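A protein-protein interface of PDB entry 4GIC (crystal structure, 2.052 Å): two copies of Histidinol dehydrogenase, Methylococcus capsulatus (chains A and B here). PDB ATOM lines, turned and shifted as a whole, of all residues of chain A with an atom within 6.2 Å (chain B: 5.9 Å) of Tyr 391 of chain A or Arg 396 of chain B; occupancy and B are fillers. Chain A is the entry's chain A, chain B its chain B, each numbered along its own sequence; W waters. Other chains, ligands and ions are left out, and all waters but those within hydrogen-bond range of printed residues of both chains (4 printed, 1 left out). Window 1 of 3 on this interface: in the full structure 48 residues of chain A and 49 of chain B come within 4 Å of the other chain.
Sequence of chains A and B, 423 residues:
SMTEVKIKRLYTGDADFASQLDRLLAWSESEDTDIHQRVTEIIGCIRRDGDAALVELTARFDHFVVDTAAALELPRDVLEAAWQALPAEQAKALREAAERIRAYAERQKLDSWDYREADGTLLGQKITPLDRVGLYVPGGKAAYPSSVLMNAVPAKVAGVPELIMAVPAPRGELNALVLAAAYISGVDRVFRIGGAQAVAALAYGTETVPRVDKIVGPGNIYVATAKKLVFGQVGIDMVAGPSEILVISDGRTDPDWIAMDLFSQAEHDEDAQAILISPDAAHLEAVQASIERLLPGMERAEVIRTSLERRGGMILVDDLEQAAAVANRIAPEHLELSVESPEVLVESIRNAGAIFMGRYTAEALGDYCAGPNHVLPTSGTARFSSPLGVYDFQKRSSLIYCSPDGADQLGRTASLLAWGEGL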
ATOM      1  N   GLN A 108      10.891 -21.935  16.544  1.00  0.00           N
ATOM      2  CA  GLN A 108      10.588 -23.310  16.908  1.00  0.00           C
ATOM      3  C   GLN A 108       9.691 -23.403  18.139  1.00  0.00           C
ATOM      4  O   GLN A 108       9.239 -24.478  18.508  1.00  0.00           O
ATOM      5  CB  GLN A 108      11.902 -24.057  17.142  1.00  0.00           C
ATOM      6  CG  GLN A 108      12.590 -24.431  15.833  1.00  0.00           C
ATOM      7  CD  GLN A 108      13.766 -25.357  16.034  1.00  0.00           C
ATOM      8  OE1 GLN A 108      14.585 -25.149  16.934  1.00  0.00           O
ATOM      9  NE2 GLN A 108      13.859 -26.394  15.194  1.00  0.00           N
ATOM     10  N   LYS A 109       9.409 -22.263  18.755  1.00  0.00           N
ATOM     11  CA  LYS A 109       8.735 -22.233  20.050  1.00  0.00           C
ATOM     12  C   LYS A 109       7.310 -22.801  19.961  1.00  0.00           C
ATOM     13  O   LYS A 109       6.562 -22.485  19.031  1.00  0.00           O
ATOM     14  CB  LYS A 109       8.700 -20.808  20.576  1.00  0.00           C
ATOM     15  CG  LYS A 109       8.255 -20.700  22.022  1.00  0.00           C
ATOM     16  CD  LYS A 109       8.245 -19.246  22.465  1.00  0.00           C
ATOM     17  CE  LYS A 109       7.784 -19.125  23.906  1.00  0.00           C
ATOM     18  NZ  LYS A 109       7.576 -17.701  24.279  1.00  0.00           N
ATOM     19  N   LEU A 110       6.942 -23.658  20.909  1.00  0.00           N
ATOM     20  CA  LEU A 110       5.597 -24.246  20.902  1.00  0.00           C
ATOM     21  C   LEU A 110       4.588 -23.265  21.493  1.00  0.00           C
ATOM     22  O   LEU A 110       4.902 -22.580  22.464  1.00  0.00           O
ATOM     23  CB  LEU A 110       5.579 -25.547  21.706  1.00  0.00           C
ATOM     24  CG  LEU A 110       6.478 -26.656  21.159  1.00  0.00           C
ATOM     25  CD1 LEU A 110       6.428 -27.863  22.074  1.00  0.00           C
ATOM     26  CD2 LEU A 110       6.061 -27.035  19.751  1.00  0.00           C
ATOM     27  N   PRO A 154      18.030 -21.293  24.072  1.00  0.00           N
ATOM     28  CA  PRO A 154      16.695 -21.876  23.854  1.00  0.00           C
ATOM     29  C   PRO A 154      15.871 -22.034  25.140  1.00  0.00           C
ATOM     30  O   PRO A 154      14.657 -21.813  25.115  1.00  0.00           O
ATOM     31  CB  PRO A 154      17.012 -23.244  23.238  1.00  0.00           C
ATOM     32  CG  PRO A 154      18.350 -23.039  22.565  1.00  0.00           C
ATOM     33  CD  PRO A 154      19.100 -22.140  23.501  1.00  0.00           C
ATOM     34  N   ALA A 158      12.199 -20.398  25.671  1.00  0.00           N
ATOM     35  CA  ALA A 158      11.076 -21.218  26.148  1.00  0.00           C
ATOM     36  C   ALA A 158      10.365 -20.579  27.346  1.00  0.00           C
ATOM     37  O   ALA A 158       9.181 -20.847  27.576  1.00  0.00           O
ATOM     38  CB  ALA A 158      11.557 -22.592  26.519  1.00  0.00           C
ATOM     39  N   ALA A 352      19.071 -37.266   9.289  1.00  0.00           N
ATOM     40  CA  ALA A 352      20.266 -36.447   9.477  1.00  0.00           C
ATOM     41  C   ALA A 352      19.981 -35.338  10.493  1.00  0.00           C
ATOM     42  O   ALA A 352      18.933 -34.698  10.422  1.00  0.00           O
ATOM     43  CB  ALA A 352      20.690 -35.843   8.139  1.00  0.00           C
ATOM     44  N   GLY A 353      20.918 -35.078  11.407  1.00  0.00           N
ATOM     45  CA  GLY A 353      20.739 -33.998  12.366  1.00  0.00           C
ATOM     46  C   GLY A 353      20.660 -32.624  11.710  1.00  0.00           C
ATOM     47  O   GLY A 353      19.739 -31.842  11.965  1.00  0.00           O
ATOM     48  N   PRO A 377      21.808 -34.805  16.975  1.00  0.00           N
ATOM     49  CA  PRO A 377      21.809 -36.225  17.351  1.00  0.00           C
ATOM     50  C   PRO A 377      22.921 -36.988  16.638  1.00  0.00           C
ATOM     51  O   PRO A 377      23.096 -36.825  15.430  1.00  0.00           O
ATOM     52  CB  PRO A 377      20.435 -36.725  16.874  1.00  0.00           C
ATOM     53  CG  PRO A 377      20.055 -35.786  15.759  1.00  0.00           C
ATOM     54  CD  PRO A 377      20.660 -34.443  16.115  1.00  0.00           C
ATOM     55  N   SER A 385      15.574 -38.979  16.610  1.00  0.00           N
ATOM     56  CA  SER A 385      15.726 -37.814  17.502  1.00  0.00           C
ATOM     57  C   SER A 385      15.868 -36.530  16.704  1.00  0.00           C
ATOM     58  O   SER A 385      16.326 -36.564  15.563  1.00  0.00           O
ATOM     59  CB  SER A 385      17.019 -37.918  18.323  1.00  0.00           C
ATOM     60  OG  SER A 385      17.206 -39.207  18.854  1.00  0.00           O
ATOM     61  N   SER A 386      15.541 -35.405  17.336  1.00  0.00           N
ATOM     62  CA  SER A 386      15.779 -34.072  16.785  1.00  0.00           C
ATOM     63  C   SER A 386      16.964 -33.424  17.513  1.00  0.00           C
ATOM     64  O   SER A 386      17.377 -33.893  18.579  1.00  0.00           O
ATOM     65  CB  SER A 386      14.532 -33.207  16.987  1.00  0.00           C
ATOM     66  OG  SER A 386      13.421 -33.802  16.338  1.00  0.00           O
ATOM     67  N   PRO A 387      17.513 -32.335  16.946  1.00  0.00           N
ATOM     68  CA  PRO A 387      18.482 -31.567  17.721  1.00  0.00           C
ATOM     69  C   PRO A 387      17.828 -31.031  18.982  1.00  0.00           C
ATOM     70  O   PRO A 387      16.602 -30.892  19.038  1.00  0.00           O
ATOM     71  CB  PRO A 387      18.796 -30.373  16.802  1.00  0.00           C
ATOM     72  CG  PRO A 387      18.492 -30.844  15.455  1.00  0.00           C
ATOM     73  CD  PRO A 387      17.327 -31.773  15.598  1.00  0.00           C
ATOM     74  N   LEU A 388      18.651 -30.732  19.975  1.00  0.00           N
ATOM     75  CA  LEU A 388      18.219 -29.982  21.141  1.00  0.00           C
ATOM     76  C   LEU A 388      17.671 -28.629  20.659  1.00  0.00           C
ATOM     77  O   LEU A 388      18.281 -27.953  19.826  1.00  0.00           O
ATOM     78  CB  LEU A 388      19.418 -29.773  22.073  1.00  0.00           C
ATOM     79  CG  LEU A 388      19.277 -29.271  23.518  1.00  0.00           C
ATOM     80  CD1 LEU A 388      19.001 -27.785  23.581  1.00  0.00           C
ATOM     81  CD2 LEU A 388      18.222 -30.061  24.270  1.00  0.00           C
ATOM     82  N   GLY A 389      16.497 -28.244  21.145  1.00  0.00           N
ATOM     83  CA  GLY A 389      15.958 -26.937  20.811  1.00  0.00           C
ATOM     84  C   GLY A 389      15.028 -26.408  21.893  1.00  0.00           C
ATOM     85  O   GLY A 389      14.849 -27.040  22.946  1.00  0.00           O
ATOM     86  N   VAL A 390      14.388 -25.284  21.590  1.00  0.00           N
ATOM     87  CA  VAL A 390      13.499 -24.618  22.514  1.00  0.00           C
ATOM     88  C   VAL A 390      12.430 -25.585  23.037  1.00  0.00           C
ATOM     89  O   VAL A 390      12.106 -25.554  24.226  1.00  0.00           O
ATOM     90  CB  VAL A 390      12.864 -23.362  21.862  1.00  0.00           C
ATOM     91  CG1 VAL A 390      12.017 -23.758  20.648  1.00  0.00           C
ATOM     92  CG2 VAL A 390      12.012 -22.602  22.866  1.00  0.00           C
ATOM     93  N   TYR A 391      11.929 -26.463  22.163  1.00  0.00           N
ATOM     94  CA  TYR A 391      10.859 -27.406  22.487  1.00  0.00           C
ATOM     95  C   TYR A 391      11.265 -28.372  23.584  1.00  0.00           C
ATOM     96  O   TYR A 391      10.409 -28.906  24.280  1.00  0.00           O
ATOM     97  CB  TYR A 391      10.422 -28.195  21.238  1.00  0.00           C
ATOM     98  CG  TYR A 391      11.599 -28.516  20.344  1.00  0.00           C
ATOM     99  CD1 TYR A 391      12.387 -29.636  20.569  1.00  0.00           C
ATOM    100  CD2 TYR A 391      11.951 -27.670  19.306  1.00  0.00           C
ATOM    101  CE1 TYR A 391      13.480 -29.919  19.762  1.00  0.00           C
ATOM    102  CE2 TYR A 391      13.034 -27.940  18.514  1.00  0.00           C
ATOM    103  CZ  TYR A 391      13.798 -29.062  18.744  1.00  0.00           C
ATOM    104  OH  TYR A 391      14.881 -29.320  17.942  1.00  0.00           O
ATOM    105  N   ASP A 392      12.565 -28.604  23.741  1.00  0.00           N
ATOM    106  CA  ASP A 392      13.016 -29.499  24.797  1.00  0.00           C
ATOM    107  C   ASP A 392      12.960 -28.878  26.189  1.00  0.00           C
ATOM    108  O   ASP A 392      13.161 -29.574  27.182  1.00  0.00           O
ATOM    109  CB  ASP A 392      14.426 -30.005  24.505  1.00  0.00           C
ATOM    110  CG  ASP A 392      14.472 -30.877  23.253  1.00  0.00           C
ATOM    111  OD1 ASP A 392      13.712 -31.868  23.189  1.00  0.00           O
ATOM    112  OD2 ASP A 392      15.257 -30.562  22.337  1.00  0.00           O
ATOM    113  N   PHE A 393      12.689 -27.580  26.264  1.00  0.00           N
ATOM    114  CA  PHE A 393      12.591 -26.904  27.563  1.00  0.00           C
ATOM    115  C   PHE A 393      11.159 -26.468  27.819  1.00  0.00           C
ATOM    116  O   PHE A 393      10.873 -25.715  28.754  1.00  0.00           O
ATOM    117  CB  PHE A 393      13.548 -25.723  27.615  1.00  0.00           C
ATOM    118  CG  PHE A 393      14.984 -26.120  27.403  1.00  0.00           C
ATOM    119  CD1 PHE A 393      15.701 -26.754  28.411  1.00  0.00           C
ATOM    120  CD2 PHE A 393      15.596 -25.924  26.178  1.00  0.00           C
ATOM    121  CE1 PHE A 393      17.039 -27.155  28.217  1.00  0.00           C
ATOM    122  CE2 PHE A 393      16.936 -26.322  25.970  1.00  0.00           C
ATOM    123  CZ  PHE A 393      17.657 -26.937  26.992  1.00  0.00           C
ATOM    124  N   GLN A 394      10.273 -26.958  26.944  1.00  0.00           N
ATOM    125  CA  GLN A 394       8.840 -26.780  27.059  1.00  0.00           C
ATOM    126  C   GLN A 394       8.198 -28.147  27.223  1.00  0.00           C
ATOM    127  O   GLN A 394       8.782 -29.176  26.852  1.00  0.00           O
ATOM    128  CB  GLN A 394       8.273 -26.147  25.778  1.00  0.00           C
ATOM    129  CG  GLN A 394       8.772 -24.753  25.470  1.00  0.00           C
ATOM    130  CD  GLN A 394       8.163 -24.196  24.200  1.00  0.00           C
ATOM    131  OE1 GLN A 394       8.460 -24.651  23.077  1.00  0.00           O
ATOM    132  NE2 GLN A 394       7.301 -23.199  24.365  1.00  0.00           N
ATOM    133  N   LYS A 395       6.970 -28.153  27.721  1.00  0.00           N
ATOM    134  CA  LYS A 395       6.214 -29.384  27.780  1.00  0.00           C
ATOM    135  C   LYS A 395       4.745 -29.065  27.501  1.00  0.00           C
ATOM    136  O   LYS A 395       4.298 -27.906  27.678  1.00  0.00           O
ATOM    137  CB  LYS A 395       6.411 -30.098  29.117  1.00  0.00           C
ATOM    138  CG  LYS A 395       6.016 -29.272  30.328  1.00  0.00           C
ATOM    139  CD  LYS A 395       6.387 -29.993  31.604  1.00  0.00           C
ATOM    140  CE  LYS A 395       6.276 -29.093  32.831  1.00  0.00           C
ATOM    141  NZ  LYS A 395       4.930 -28.464  32.978  1.00  0.00           N
ATOM    142  N   ARG A 396       4.008 -30.080  27.049  1.00  0.00           N
ATOM    143  CA  ARG A 396       2.594 -29.938  26.719  1.00  0.00           C
ATOM    144  C   ARG A 396       1.721 -30.666  27.729  1.00  0.00           C
ATOM    145  O   ARG A 396       2.092 -31.736  28.222  1.00  0.00           O
ATOM    146  CB  ARG A 396       2.308 -30.530  25.338  1.00  0.00           C
ATOM    147  CG  ARG A 396       3.355 -30.211  24.294  1.00  0.00           C
ATOM    148  CD  ARG A 396       3.106 -31.050  23.064  1.00  0.00           C
ATOM    149  NE  ARG A 396       4.213 -31.024  22.120  1.00  0.00           N
ATOM    150  CZ  ARG A 396       4.113 -30.575  20.873  1.00  0.00           C
ATOM    151  NH1 ARG A 396       2.950 -30.101  20.417  1.00  0.00           N
ATOM    152  NH2 ARG A 396       5.171 -30.611  20.075  1.00  0.00           N
ATOM    153  N   LEU B 110       3.851 -31.273  13.455  1.00  0.00           N
ATOM    154  CA  LEU B 110       4.918 -30.324  13.181  1.00  0.00           C
ATOM    155  C   LEU B 110       5.040 -30.135  11.664  1.00  0.00           C
ATOM    156  O   LEU B 110       4.790 -31.079  10.900  1.00  0.00           O
ATOM    157  CB  LEU B 110       6.230 -30.830  13.790  1.00  0.00           C
ATOM    158  CG  LEU B 110       6.320 -30.985  15.316  1.00  0.00           C
ATOM    159  CD1 LEU B 110       7.626 -31.661  15.709  1.00  0.00           C
ATOM    160  CD2 LEU B 110       6.227 -29.617  15.996  1.00  0.00           C
ATOM    161  N   TRP B 113       9.611 -25.600   7.628  1.00  0.00           N
ATOM    162  CA  TRP B 113       9.617 -24.200   7.219  1.00  0.00           C
ATOM    163  C   TRP B 113      11.047 -23.737   7.009  1.00  0.00           C
ATOM    164  O   TRP B 113      11.989 -24.443   7.353  1.00  0.00           O
ATOM    165  CB  TRP B 113       8.904 -23.285   8.227  1.00  0.00           C
ATOM    166  CG  TRP B 113       9.284 -23.543   9.652  1.00  0.00           C
ATOM    167  CD1 TRP B 113       8.556 -24.241  10.568  1.00  0.00           C
ATOM    168  CD2 TRP B 113      10.477 -23.112  10.330  1.00  0.00           C
ATOM    169  NE1 TRP B 113       9.220 -24.272  11.777  1.00  0.00           N
ATOM    170  CE2 TRP B 113      10.403 -23.590  11.654  1.00  0.00           C
ATOM    171  CE3 TRP B 113      11.601 -22.374   9.946  1.00  0.00           C
ATOM    172  CZ2 TRP B 113      11.406 -23.349  12.597  1.00  0.00           C
ATOM    173  CZ3 TRP B 113      12.601 -22.136  10.886  1.00  0.00           C
ATOM    174  CH2 TRP B 113      12.495 -22.626  12.191  1.00  0.00           C
ATOM    175  N   GLN B 125      13.922 -25.779   8.996  1.00  0.00           N
ATOM    176  CA  GLN B 125      13.576 -26.925   9.785  1.00  0.00           C
ATOM    177  C   GLN B 125      12.863 -27.856   8.835  1.00  0.00           C
ATOM    178  O   GLN B 125      11.846 -27.490   8.220  1.00  0.00           O
ATOM    179  CB  GLN B 125      12.631 -26.521  10.926  1.00  0.00           C
ATOM    180  CG  GLN B 125      11.996 -27.705  11.611  1.00  0.00           C
ATOM    181  CD  GLN B 125      11.051 -27.309  12.729  1.00  0.00           C
ATOM    182  OE1 GLN B 125      11.478 -27.037  13.853  1.00  0.00           O
ATOM    183  NE2 GLN B 125       9.754 -27.299  12.430  1.00  0.00           N
ATOM    184  N   LYS B 126      13.420 -29.045   8.700  1.00  0.00           N
ATOM    185  CA  LYS B 126      12.863 -30.071   7.853  1.00  0.00           C
ATOM    186  C   LYS B 126      12.280 -31.158   8.734  1.00  0.00           C
ATOM    187  O   LYS B 126      13.017 -31.833   9.453  1.00  0.00           O
ATOM    188  CB  LYS B 126      13.961 -30.655   6.968  1.00  0.00           C
ATOM    189  CG  LYS B 126      13.500 -31.775   6.027  1.00  0.00           C
ATOM    190  CD  LYS B 126      14.728 -32.397   5.371  1.00  0.00           C
ATOM    191  CE  LYS B 126      14.393 -33.217   4.145  1.00  0.00           C
ATOM    192  NZ  LYS B 126      13.499 -34.362   4.428  1.00  0.00           N
ATOM    193  N   ILE B 127      10.960 -31.325   8.662  1.00  0.00           N
ATOM    194  CA  ILE B 127      10.235 -32.337   9.435  1.00  0.00           C
ATOM    195  C   ILE B 127      10.093 -33.622   8.632  1.00  0.00           C
ATOM    196  O   ILE B 127       9.686 -33.587   7.474  1.00  0.00           O
ATOM    197  CB  ILE B 127       8.822 -31.853   9.776  1.00  0.00           C
ATOM    198  CG1 ILE B 127       8.879 -30.572  10.616  1.00  0.00           C
ATOM    199  CG2 ILE B 127       8.020 -32.962  10.477  1.00  0.00           C
ATOM    200  CD1 ILE B 127       9.626 -30.737  11.912  1.00  0.00           C
ATOM    201  N   THR B 128      10.429 -34.756   9.237  1.00  0.00           N
ATOM    202  CA  THR B 128      10.195 -36.060   8.592  1.00  0.00           C
ATOM    203  C   THR B 128       9.514 -37.008   9.565  1.00  0.00           C
ATOM    204  O   THR B 128       9.730 -36.897  10.773  1.00  0.00           O
ATOM    205  CB  THR B 128      11.517 -36.733   8.172  1.00  0.00           C
ATOM    206  OG1 THR B 128      12.392 -36.750   9.315  1.00  0.00           O
ATOM    207  CG2 THR B 128      12.196 -35.977   6.989  1.00  0.00           C
ATOM    208  N   GLN B 394       7.572 -37.869  14.708  1.00  0.00           N
ATOM    209  CA  GLN B 394       8.229 -36.965  13.768  1.00  0.00           C
ATOM    210  C   GLN B 394       9.611 -36.576  14.300  1.00  0.00           C
ATOM    211  O   GLN B 394       9.911 -36.780  15.477  1.00  0.00           O
ATOM    212  CB  GLN B 394       7.408 -35.690  13.616  1.00  0.00           C
ATOM    213  CG  GLN B 394       6.021 -35.894  13.035  1.00  0.00           C
ATOM    214  CD  GLN B 394       5.279 -34.577  12.939  1.00  0.00           C
ATOM    215  OE1 GLN B 394       4.915 -33.981  13.951  1.00  0.00           O
ATOM    216  NE2 GLN B 394       5.069 -34.108  11.722  1.00  0.00           N
ATOM    217  N   LYS B 395      10.463 -36.031  13.435  1.00  0.00           N
ATOM    218  CA  LYS B 395      11.736 -35.449  13.882  1.00  0.00           C
ATOM    219  C   LYS B 395      12.127 -34.284  13.003  1.00  0.00           C
ATOM    220  O   LYS B 395      11.631 -34.154  11.867  1.00  0.00           O
ATOM    221  CB  LYS B 395      12.837 -36.505  13.948  1.00  0.00           C
ATOM    222  CG  LYS B 395      13.035 -37.256  12.636  1.00  0.00           C
ATOM    223  CD  LYS B 395      13.944 -38.446  12.864  1.00  0.00           C
ATOM    224  CE  LYS B 395      13.894 -39.391  11.678  1.00  0.00           C
ATOM    225  NZ  LYS B 395      14.187 -38.656  10.432  1.00  0.00           N
ATOM    226  N   ARG B 396      13.013 -33.437  13.526  1.00  0.00           N
ATOM    227  CA  ARG B 396      13.454 -32.238  12.829  1.00  0.00           C
ATOM    228  C   ARG B 396      14.907 -32.375  12.410  1.00  0.00           C
ATOM    229  O   ARG B 396      15.718 -32.987  13.107  1.00  0.00           O
ATOM    230  CB  ARG B 396      13.336 -31.016  13.744  1.00  0.00           C
ATOM    231  CG  ARG B 396      12.109 -31.034  14.650  1.00  0.00           C
ATOM    232  CD  ARG B 396      12.293 -30.076  15.813  1.00  0.00           C
ATOM    233  NE  ARG B 396      11.178 -30.111  16.750  1.00  0.00           N
ATOM    234  CZ  ARG B 396      10.271 -29.143  16.858  1.00  0.00           C
ATOM    235  NH1 ARG B 396      10.349 -28.057  16.089  1.00  0.00           N
ATOM    236  NH2 ARG B 396       9.294 -29.250  17.750  1.00  0.00           N
ATOM    237  N   SER B 397      15.224 -31.782  11.272  1.00  0.00           N
ATOM    238  CA  SER B 397      16.580 -31.717  10.784  1.00  0.00           C
ATOM    239  C   SER B 397      16.808 -30.244  10.541  1.00  0.00           C
ATOM    240  O   SER B 397      15.937 -29.570   9.977  1.00  0.00           O
ATOM    241  CB  SER B 397      16.697 -32.475   9.460  1.00  0.00           C
ATOM    242  OG  SER B 397      16.605 -33.869   9.679  1.00  0.00           O
ATOM    243  N   SER B 398      17.952 -29.723  10.966  1.00  0.00           N
ATOM    244  CA  SER B 398      18.295 -28.364  10.617  1.00  0.00           C
ATOM    245  C   SER B 398      18.773 -28.294   9.166  1.00  0.00           C
ATOM    246  O   SER B 398      19.604 -29.096   8.732  1.00  0.00           O
ATOM    247  CB  SER B 398      19.372 -27.848  11.567  1.00  0.00           C
ATOM    248  OG  SER B 398      18.902 -27.996  12.893  1.00  0.00           O
HETATM  249  O   HOH W   1       8.306 -26.659  17.241  1.00  0.00           O
HETATM  250  O   HOH W   2      16.783 -37.049  11.096  1.00  0.00           O
HETATM  251  O   HOH W   3      12.260 -35.739  17.620  1.00  0.00           O
HETATM  252  O   HOH W   4       8.144 -31.169  19.911  1.00  0.00           O
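OG of Ser 397 of chain B is in hydrogen-bond range of O of Ala 352 of chain A, at 2.6 Å. The backbone carbonyl oxygen (O) of Gly 353 of chain A sits at hydrogen-bond distance from the backbone NH (N) of Ser 398 of chain B, at 2.9 Å. The side-chain hydroxyl (OG) of Ser 386 of chain A is in hydrogen-bond range of the backbone NH (N) of Arg 396 of chain B. OE1 of Gln 125 of chain B lies within hydrogen-bond range of NE2 of Gln 108 of chain A (2.8 Å).
The backbone carbonyl oxygen (O) of Lys 126 of chain B is in hydrogen-bond range of the backbone NH (N) of Ser 397 of chain B (2.9 Å). The side-chain amide oxygen of Gln 125 of chain B sits at hydrogen-bond distance from the guanidinium group of Arg 396 of chain B (2.7 Å). The backbone carbonyl oxygen (O) of Pro 387 of chain A sits at hydrogen-bond distance from the side-chain hydroxyl (OH) of Tyr 391 of chain A. The side-chain amino group of Lys 395 of chain B lies within hydrogen-bond range of the side-chain hydroxyl of Thr 128 of chain B (2.8 Å). The backbone carbonyl oxygen (O) of Trp 113 of chain B is in hydrogen-bond range of the backbone NH (N) of Gln 125 of chain B (2.9 Å).
Among the printed residues, merely in contact across the chains: Gln 108 of chain A with Trp 113 of chain B (3.6 Å), Gln 108 of chain A with Arg 396 of chain B (3.99 Å), Gly 353 of chain A with Ser 397 of chain B (3.4 Å), Ser 385 of chain A with Lys 395 of chain B (3.8 Å), Ser 386 of chain A with Lys 395 of chain B (3.4 Å), Pro 387 of chain A with Arg 396 of chain B (3.2 Å), Pro 387 of chain A with Ser 398 of chain B (3.9 Å) and Tyr 391 of chain A with Arg 396 of chain B (3.3 Å).
Printed residues of chain A within 4 Å of Arg 396 of chain B: Gln 108 (3.99 Å), Ser 386 (2.9 Å), Pro 387 (3.2 Å) and Tyr 391 (3.3 Å). Of the printed residues of chain B, Pro 387 of chain A touches Arg 396 and Ser 398. Of the printed residues of chain A, Ser 398 of chain B touches Gly 353 and Pro 387. Phe 393 of chain A touches none of the printed residues of chain B. The nearest printed residue of chain A that does not touch Trp 113 of chain B is Lys 109 of chain A (6.6 Å).
Hydrophobic or aromatic side chains of chain B that line the printed part of chain A: Trp 113. Of the 20 printed residues of chain A, 7 touch a printed residue of chain B. Hydrophobic or aromatic side chains of chain A within 4 Å of the printed part of chain B: Pro 387 and Tyr 391. Among the printed residues, 12 pairs touch across the chains.
Positions printed for both chains: 110, 394, 395 and 396.
Water W3 bridges the side-chain hydroxyl (OG) of Ser 386 of chain A (2.6 Å) and the backbone carbonyl oxygen (O) of Gln 394 of chain B (3.3 Å). Water W1 lies within hydrogen-bond range of O of Gln 108 of chain A and NH1 of Arg 396 of chain B. Water W2 lies within hydrogen-bond range of the backbone NH of Ala 352 of chain A, the side-chain amino group of Lys 395 of chain B and the side-chain hydroxyl of Ser 397 of chain B. Water W4 lies within hydrogen-bond range of the guanidinium group (NH2) of Arg 396 of chain A (3.0 Å) and the guanidinium group (NH2) of Arg 396 of chain B (3.1 Å).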
